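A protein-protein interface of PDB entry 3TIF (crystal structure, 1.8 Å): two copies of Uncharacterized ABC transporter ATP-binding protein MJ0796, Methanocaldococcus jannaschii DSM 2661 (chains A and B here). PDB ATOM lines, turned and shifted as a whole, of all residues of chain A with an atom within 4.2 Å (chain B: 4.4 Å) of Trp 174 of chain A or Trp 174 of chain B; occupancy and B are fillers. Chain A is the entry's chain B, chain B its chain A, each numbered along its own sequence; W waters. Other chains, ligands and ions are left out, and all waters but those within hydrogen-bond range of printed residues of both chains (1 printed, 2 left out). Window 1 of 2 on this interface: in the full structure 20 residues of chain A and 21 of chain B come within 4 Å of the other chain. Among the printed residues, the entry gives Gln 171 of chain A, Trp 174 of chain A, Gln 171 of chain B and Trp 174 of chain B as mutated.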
ATOM      1  N   GLN A  90     -22.413 -28.623 -19.404  1.00  0.00           N
ATOM      2  CA  GLN A  90     -22.292 -28.179 -20.798  1.00  0.00           C
ATOM      3  C   GLN A  90     -22.634 -29.295 -21.779  1.00  0.00           C
ATOM      4  O   GLN A  90     -23.317 -29.070 -22.777  1.00  0.00           O
ATOM      5  CB  GLN A  90     -20.889 -27.648 -21.090  1.00  0.00           C
ATOM      6  CG  GLN A  90     -20.771 -26.953 -22.452  1.00  0.00           C
ATOM      7  CD  GLN A  90     -19.375 -26.440 -22.686  1.00  0.00           C
ATOM      8  OE1 GLN A  90     -18.546 -26.519 -21.793  1.00  0.00           O
ATOM      9  NE2 GLN A  90     -19.100 -25.915 -23.878  1.00  0.00           N
ATOM     10  N   PHE A  92     -24.271 -32.123 -20.752  1.00  0.00           N
ATOM     11  CA  PHE A  92     -25.412 -32.847 -20.162  1.00  0.00           C
ATOM     12  C   PHE A  92     -25.052 -33.924 -19.146  1.00  0.00           C
ATOM     13  O   PHE A  92     -25.613 -33.957 -18.050  1.00  0.00           O
ATOM     14  CB  PHE A  92     -26.323 -33.428 -21.254  1.00  0.00           C
ATOM     15  CG  PHE A  92     -26.537 -32.499 -22.404  1.00  0.00           C
ATOM     16  CD1 PHE A  92     -26.697 -32.981 -23.686  1.00  0.00           C
ATOM     17  CD2 PHE A  92     -26.551 -31.121 -22.199  1.00  0.00           C
ATOM     18  CE1 PHE A  92     -26.904 -32.105 -24.750  1.00  0.00           C
ATOM     19  CE2 PHE A  92     -26.749 -30.249 -23.250  1.00  0.00           C
ATOM     20  CZ  PHE A  92     -26.926 -30.739 -24.531  1.00  0.00           C
ATOM     21  N   GLN A 152     -30.700 -31.563 -23.472  1.00  0.00           N
ATOM     22  CA  GLN A 152     -30.354 -30.402 -22.664  1.00  0.00           C
ATOM     23  C   GLN A 152     -31.458 -30.114 -21.664  1.00  0.00           C
ATOM     24  O   GLN A 152     -31.199 -29.758 -20.516  1.00  0.00           O
ATOM     25  CB  GLN A 152     -30.134 -29.171 -23.542  1.00  0.00           C
ATOM     26  CG  GLN A 152     -29.672 -27.972 -22.765  1.00  0.00           C
ATOM     27  CD  GLN A 152     -28.861 -27.018 -23.618  1.00  0.00           C
ATOM     28  OE1 GLN A 152     -29.328 -26.561 -24.658  1.00  0.00           O
ATOM     29  NE2 GLN A 152     -27.633 -26.727 -23.194  1.00  0.00           N
ATOM     30  N   GLN A 171     -23.882 -22.945 -20.114  1.00  0.00           N
ATOM     31  CA  GLN A 171     -24.409 -22.796 -21.468  1.00  0.00           C
ATOM     32  C   GLN A 171     -25.750 -23.524 -21.633  1.00  0.00           C
ATOM     33  O   GLN A 171     -25.912 -24.351 -22.529  1.00  0.00           O
ATOM     34  CB  GLN A 171     -23.348 -23.269 -22.482  1.00  0.00           C
ATOM     35  CG  GLN A 171     -21.978 -22.623 -22.200  1.00  0.00           C
ATOM     36  CD  GLN A 171     -20.894 -22.987 -23.200  1.00  0.00           C
ATOM     37  OE1 GLN A 171     -21.184 -23.346 -24.325  1.00  0.00           O
ATOM     38  NE2 GLN A 171     -19.628 -22.881 -22.779  1.00  0.00           N
ATOM     39  N   PRO A 172     -26.732 -23.196 -20.780  1.00  0.00           N
ATOM     40  CA  PRO A 172     -27.947 -24.020 -20.699  1.00  0.00           C
ATOM     41  C   PRO A 172     -28.900 -23.928 -21.911  1.00  0.00           C
ATOM     42  O   PRO A 172     -29.868 -24.675 -21.979  1.00  0.00           O
ATOM     43  CB  PRO A 172     -28.636 -23.493 -19.430  1.00  0.00           C
ATOM     44  CG  PRO A 172     -28.154 -22.100 -19.287  1.00  0.00           C
ATOM     45  CD  PRO A 172     -26.727 -22.111 -19.779  1.00  0.00           C
ATOM     46  N   THR A 173     -28.630 -23.026 -22.842  1.00  0.00           N
ATOM     47  CA  THR A 173     -29.506 -22.868 -23.995  1.00  0.00           C
ATOM     48  C   THR A 173     -28.822 -23.203 -25.312  1.00  0.00           C
ATOM     49  O   THR A 173     -29.427 -23.034 -26.367  1.00  0.00           O
ATOM     50  CB  THR A 173     -30.023 -21.417 -24.123  1.00  0.00           C
ATOM     51  OG1 THR A 173     -28.912 -20.549 -24.377  1.00  0.00           O
ATOM     52  CG2 THR A 173     -30.729 -20.984 -22.854  1.00  0.00           C
ATOM     53  N   TRP A 174     -27.576 -23.689 -25.282  1.00  0.00           N
ATOM     54  CA  TRP A 174     -26.853 -23.829 -26.548  1.00  0.00           C
ATOM     55  C   TRP A 174     -27.543 -24.703 -27.585  1.00  0.00           C
ATOM     56  O   TRP A 174     -27.424 -24.448 -28.787  1.00  0.00           O
ATOM     57  CB  TRP A 174     -25.398 -24.299 -26.349  1.00  0.00           C
ATOM     58  CG  TRP A 174     -25.185 -25.741 -25.968  1.00  0.00           C
ATOM     59  CD1 TRP A 174     -24.885 -26.230 -24.714  1.00  0.00           C
ATOM     60  CD2 TRP A 174     -25.165 -26.884 -26.844  1.00  0.00           C
ATOM     61  NE1 TRP A 174     -24.707 -27.584 -24.765  1.00  0.00           N
ATOM     62  CE2 TRP A 174     -24.873 -28.015 -26.068  1.00  0.00           C
ATOM     63  CE3 TRP A 174     -25.355 -27.049 -28.228  1.00  0.00           C
ATOM     64  CZ2 TRP A 174     -24.773 -29.307 -26.600  1.00  0.00           C
ATOM     65  CZ3 TRP A 174     -25.266 -28.340 -28.765  1.00  0.00           C
ATOM     66  CH2 TRP A 174     -24.970 -29.449 -27.953  1.00  0.00           C
ATOM     67  N   ALA A 175     -28.238 -25.738 -27.124  1.00  0.00           N
ATOM     68  CA  ALA A 175     -28.866 -26.710 -28.023  1.00  0.00           C
ATOM     69  C   ALA A 175     -30.319 -26.381 -28.335  1.00  0.00           C
ATOM     70  O   ALA A 175     -31.022 -27.197 -28.932  1.00  0.00           O
ATOM     71  CB  ALA A 175     -28.776 -28.101 -27.444  1.00  0.00           C
ATOM     72  N   LEU A 176     -30.761 -25.202 -27.926  1.00  0.00           N
ATOM     73  CA  LEU A 176     -32.168 -24.848 -28.041  1.00  0.00           C
ATOM     74  C   LEU A 176     -32.413 -23.729 -29.045  1.00  0.00           C
ATOM     75  O   LEU A 176     -31.618 -22.806 -29.168  1.00  0.00           O
ATOM     76  CB  LEU A 176     -32.706 -24.418 -26.669  1.00  0.00           C
ATOM     77  CG  LEU A 176     -32.613 -25.430 -25.526  1.00  0.00           C
ATOM     78  CD1 LEU A 176     -33.133 -24.802 -24.209  1.00  0.00           C
ATOM     79  CD2 LEU A 176     -33.376 -26.707 -25.876  1.00  0.00           C
ATOM     80  N   GLN B  90     -22.386 -32.757 -33.575  1.00  0.00           N
ATOM     81  CA  GLN B  90     -22.937 -31.816 -32.602  1.00  0.00           C
ATOM     82  C   GLN B  90     -22.218 -31.924 -31.260  1.00  0.00           C
ATOM     83  O   GLN B  90     -21.972 -30.927 -30.593  1.00  0.00           O
ATOM     84  CB  GLN B  90     -24.446 -32.045 -32.417  1.00  0.00           C
ATOM     85  CG  GLN B  90     -25.120 -31.014 -31.528  1.00  0.00           C
ATOM     86  CD  GLN B  90     -26.623 -31.259 -31.362  1.00  0.00           C
ATOM     87  OE1 GLN B  90     -27.186 -32.150 -31.987  1.00  0.00           O
ATOM     88  NE2 GLN B  90     -27.271 -30.457 -30.522  1.00  0.00           N
ATOM     89  N   GLN B  91     -21.876 -33.143 -30.868  1.00  0.00           N
ATOM     90  CA  GLN B  91     -21.107 -33.333 -29.639  1.00  0.00           C
ATOM     91  C   GLN B  91     -19.716 -33.933 -29.864  1.00  0.00           C
ATOM     92  O   GLN B  91     -19.137 -34.584 -28.990  1.00  0.00           O
ATOM     93  CB  GLN B  91     -21.936 -34.019 -28.548  1.00  0.00           C
ATOM     94  CG  GLN B  91     -22.973 -33.054 -27.921  1.00  0.00           C
ATOM     95  CD  GLN B  91     -23.853 -33.704 -26.897  1.00  0.00           C
ATOM     96  OE1 GLN B  91     -24.966 -34.137 -27.202  1.00  0.00           O
ATOM     97  NE2 GLN B  91     -23.360 -33.793 -25.665  1.00  0.00           N
ATOM     98  N   PHE B  92     -19.192 -33.647 -31.053  1.00  0.00           N
ATOM     99  CA  PHE B  92     -17.764 -33.762 -31.369  1.00  0.00           C
ATOM    100  C   PHE B  92     -17.299 -35.180 -31.644  1.00  0.00           C
ATOM    101  O   PHE B  92     -16.605 -35.425 -32.631  1.00  0.00           O
ATOM    102  CB  PHE B  92     -16.897 -33.129 -30.278  1.00  0.00           C
ATOM    103  CG  PHE B  92     -17.423 -31.815 -29.768  1.00  0.00           C
ATOM    104  CD1 PHE B  92     -17.268 -31.457 -28.434  1.00  0.00           C
ATOM    105  CD2 PHE B  92     -18.093 -30.948 -30.618  1.00  0.00           C
ATOM    106  CE1 PHE B  92     -17.761 -30.251 -27.962  1.00  0.00           C
ATOM    107  CE2 PHE B  92     -18.593 -29.748 -30.152  1.00  0.00           C
ATOM    108  CZ  PHE B  92     -18.436 -29.401 -28.820  1.00  0.00           C
ATOM    109  N   GLN B 152     -14.618 -28.585 -30.003  1.00  0.00           N
ATOM    110  CA  GLN B 152     -15.416 -28.337 -31.204  1.00  0.00           C
ATOM    111  C   GLN B 152     -14.507 -28.047 -32.398  1.00  0.00           C
ATOM    112  O   GLN B 152     -14.736 -28.539 -33.499  1.00  0.00           O
ATOM    113  CB  GLN B 152     -16.398 -27.196 -30.972  1.00  0.00           C
ATOM    114  CG  GLN B 152     -17.337 -26.954 -32.146  1.00  0.00           C
ATOM    115  CD  GLN B 152     -18.593 -26.199 -31.734  1.00  0.00           C
ATOM    116  OE1 GLN B 152     -18.510 -25.120 -31.131  1.00  0.00           O
ATOM    117  NE2 GLN B 152     -19.760 -26.762 -32.048  1.00  0.00           N
ATOM    118  N   GLN B 171     -24.310 -27.635 -35.997  1.00  0.00           N
ATOM    119  CA  GLN B 171     -24.157 -26.604 -34.978  1.00  0.00           C
ATOM    120  C   GLN B 171     -22.687 -26.336 -34.647  1.00  0.00           C
ATOM    121  O   GLN B 171     -22.287 -26.372 -33.482  1.00  0.00           O
ATOM    122  CB  GLN B 171     -24.932 -26.993 -33.716  1.00  0.00           C
ATOM    123  CG  GLN B 171     -26.440 -27.154 -33.970  1.00  0.00           C
ATOM    124  CD  GLN B 171     -27.136 -27.901 -32.848  1.00  0.00           C
ATOM    125  OE1 GLN B 171     -27.574 -29.025 -33.024  1.00  0.00           O
ATOM    126  NE2 GLN B 171     -27.209 -27.291 -31.687  1.00  0.00           N
ATOM    127  N   PRO B 172     -21.884 -26.037 -35.675  1.00  0.00           N
ATOM    128  CA  PRO B 172     -20.417 -26.030 -35.527  1.00  0.00           C
ATOM    129  C   PRO B 172     -19.869 -24.835 -34.725  1.00  0.00           C
ATOM    130  O   PRO B 172     -18.658 -24.763 -34.522  1.00  0.00           O
ATOM    131  CB  PRO B 172     -19.921 -25.942 -36.977  1.00  0.00           C
ATOM    132  CG  PRO B 172     -21.045 -25.127 -37.677  1.00  0.00           C
ATOM    133  CD  PRO B 172     -22.320 -25.646 -37.032  1.00  0.00           C
ATOM    134  N   THR B 173     -20.729 -23.917 -34.287  1.00  0.00           N
ATOM    135  CA  THR B 173     -20.261 -22.755 -33.520  1.00  0.00           C
ATOM    136  C   THR B 173     -20.848 -22.719 -32.114  1.00  0.00           C
ATOM    137  O   THR B 173     -20.671 -21.736 -31.397  1.00  0.00           O
ATOM    138  CB  THR B 173     -20.662 -21.421 -34.203  1.00  0.00           C
ATOM    139  OG1 THR B 173     -22.090 -21.312 -34.232  1.00  0.00           O
ATOM    140  CG2 THR B 173     -20.118 -21.353 -35.603  1.00  0.00           C
ATOM    141  N   TRP B 174     -21.577 -23.759 -31.724  1.00  0.00           N
ATOM    142  CA  TRP B 174     -22.374 -23.633 -30.506  1.00  0.00           C
ATOM    143  C   TRP B 174     -21.513 -23.376 -29.268  1.00  0.00           C
ATOM    144  O   TRP B 174     -21.918 -22.629 -28.363  1.00  0.00           O
ATOM    145  CB  TRP B 174     -23.322 -24.824 -30.307  1.00  0.00           C
ATOM    146  CG  TRP B 174     -22.709 -26.127 -29.866  1.00  0.00           C
ATOM    147  CD1 TRP B 174     -22.528 -27.247 -30.632  1.00  0.00           C
ATOM    148  CD2 TRP B 174     -22.268 -26.477 -28.538  1.00  0.00           C
ATOM    149  NE1 TRP B 174     -21.980 -28.260 -29.867  1.00  0.00           N
ATOM    150  CE2 TRP B 174     -21.814 -27.810 -28.579  1.00  0.00           C
ATOM    151  CE3 TRP B 174     -22.225 -25.786 -27.316  1.00  0.00           C
ATOM    152  CZ2 TRP B 174     -21.300 -28.473 -27.456  1.00  0.00           C
ATOM    153  CZ3 TRP B 174     -21.710 -26.437 -26.199  1.00  0.00           C
ATOM    154  CH2 TRP B 174     -21.267 -27.772 -26.270  1.00  0.00           C
ATOM    155  N   ALA B 175     -20.325 -23.969 -29.241  1.00  0.00           N
ATOM    156  CA  ALA B 175     -19.472 -23.885 -28.058  1.00  0.00           C
ATOM    157  C   ALA B 175     -18.450 -22.763 -28.173  1.00  0.00           C
ATOM    158  O   ALA B 175     -17.510 -22.673 -27.370  1.00  0.00           O
ATOM    159  CB  ALA B 175     -18.767 -25.240 -27.811  1.00  0.00           C
ATOM    160  N   LEU B 176     -18.635 -21.906 -29.174  1.00  0.00           N
ATOM    161  CA  LEU B 176     -17.682 -20.840 -29.454  1.00  0.00           C
ATOM    162  C   LEU B 176     -18.275 -19.468 -29.122  1.00  0.00           C
ATOM    163  O   LEU B 176     -19.459 -19.222 -29.329  1.00  0.00           O
ATOM    164  CB  LEU B 176     -17.269 -20.879 -30.935  1.00  0.00           C
ATOM    165  CG  LEU B 176     -16.654 -22.182 -31.449  1.00  0.00           C
ATOM    166  CD1 LEU B 176     -16.259 -22.060 -32.914  1.00  0.00           C
ATOM    167  CD2 LEU B 176     -15.451 -22.540 -30.607  1.00  0.00           C
HETATM  168  O   HOH W   1     -25.160 -21.886 -29.248  1.00  0.00           O
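The side-chain amide nitrogen of Gln 90 of chain B is in hydrogen-bond range of the side-chain amide oxygen of Gln 171 of chain B, at 2.9 Å.
NE2 of Gln 152 of chain B sits at hydrogen-bond distance from O of Gln 171 of chain B (2.9 Å).
OE1 of Gln 152 of chain B lies within hydrogen-bond range of N of Trp 174 of chain B (3.4 Å).
The side-chain amide nitrogen of Gln 90 of chain A sits close to the side-chain amide nitrogen of Gln 171 of chain A (3.3 Å).
NE1 of Trp 174 of chain A sits at hydrogen-bond distance from O of Gln 90 of chain A, at 2.8 Å.
OE1 of Gln 152 of chain A lies within hydrogen-bond range of N of Trp 174 of chain A, at 3.4 Å.
Trp 174 of chain B touches Gln 90 of chain A (CZ3 to NE2, 3.5 Å).
OE1 of Gln 91 of chain B touches CE1 of Phe 92 of chain A (3.7 Å).
Gln 171 of chain A touches Trp 174 of chain B.
NE2 of Gln 90 of chain B touches CZ3 of Trp 174 of chain A, 3.4 Å away.
Trp 174 of chain A touches Gln 171 of chain B.
Trp 174 of chain B touches Trp 174 of chain A (CD2 to CE3, 3.2 Å).
Printed residues of chain B within 4 Å of Trp 174 of chain A: Gln 90 (3.4 Å), Gln 171 (3.7 Å) and Trp 174 (3.2 Å).
Trp 174 of chain B touches three residues of chain A.
Of the printed residues of chain B, Phe 92 of chain A touches Gln 91.
Of the printed residues of chain A, Gln 171 of chain B touches Trp 174.
Of the printed residues of chain A, Gln 90 of chain B touches Trp 174.
Leu 176 of chain A touches none of the printed residues of chain B.
Leu 176 of chain B touches none of the printed residues of chain A.
The nearest printed residue of chain B that does not touch Trp 174 of chain A is Gln 91 of chain B (4.1 Å).
The nearest printed residue of chain A that does not touch Trp 174 of chain B is Ala 175 of chain A (5.9 Å).
Hydrophobic or aromatic side chains of chain B that line the printed part of chain A: Trp 174.
Of the 9 printed residues of chain A, 4 touch a printed residue of chain B.
Hydrophobic or aromatic side chains of chain A within 4 Å of the printed part of chain B: Phe 92 and Trp 174.
Among the printed residues, 6 pairs touch across the chains.
Among the printed residues, no Asp or Glu carboxylate lies within 4 Å of a Lys or Arg side-chain nitrogen of the other chain.
Gln 90 of chain A touches Trp 174 of chain B, and with the chains exchanged Trp 174 of chain A touches Gln 90 of chain B.
Gln 171 of chain A touches Trp 174 of chain B, and with the chains exchanged Trp 174 of chain A touches Gln 171 of chain B.
Trp 174 of chain B touches its own counterpart, Trp 174 of chain A.
9 positions are printed for both chains.
Of the 6 pairs that touch across the chains among the printed residues, 5 have their exchanged pair printed and touching as well.
Water W1 bridges the backbone carbonyl oxygen (O) of Trp 174 of chain B and the backbone carbonyl oxygen (O) of Trp 174 of chain A.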
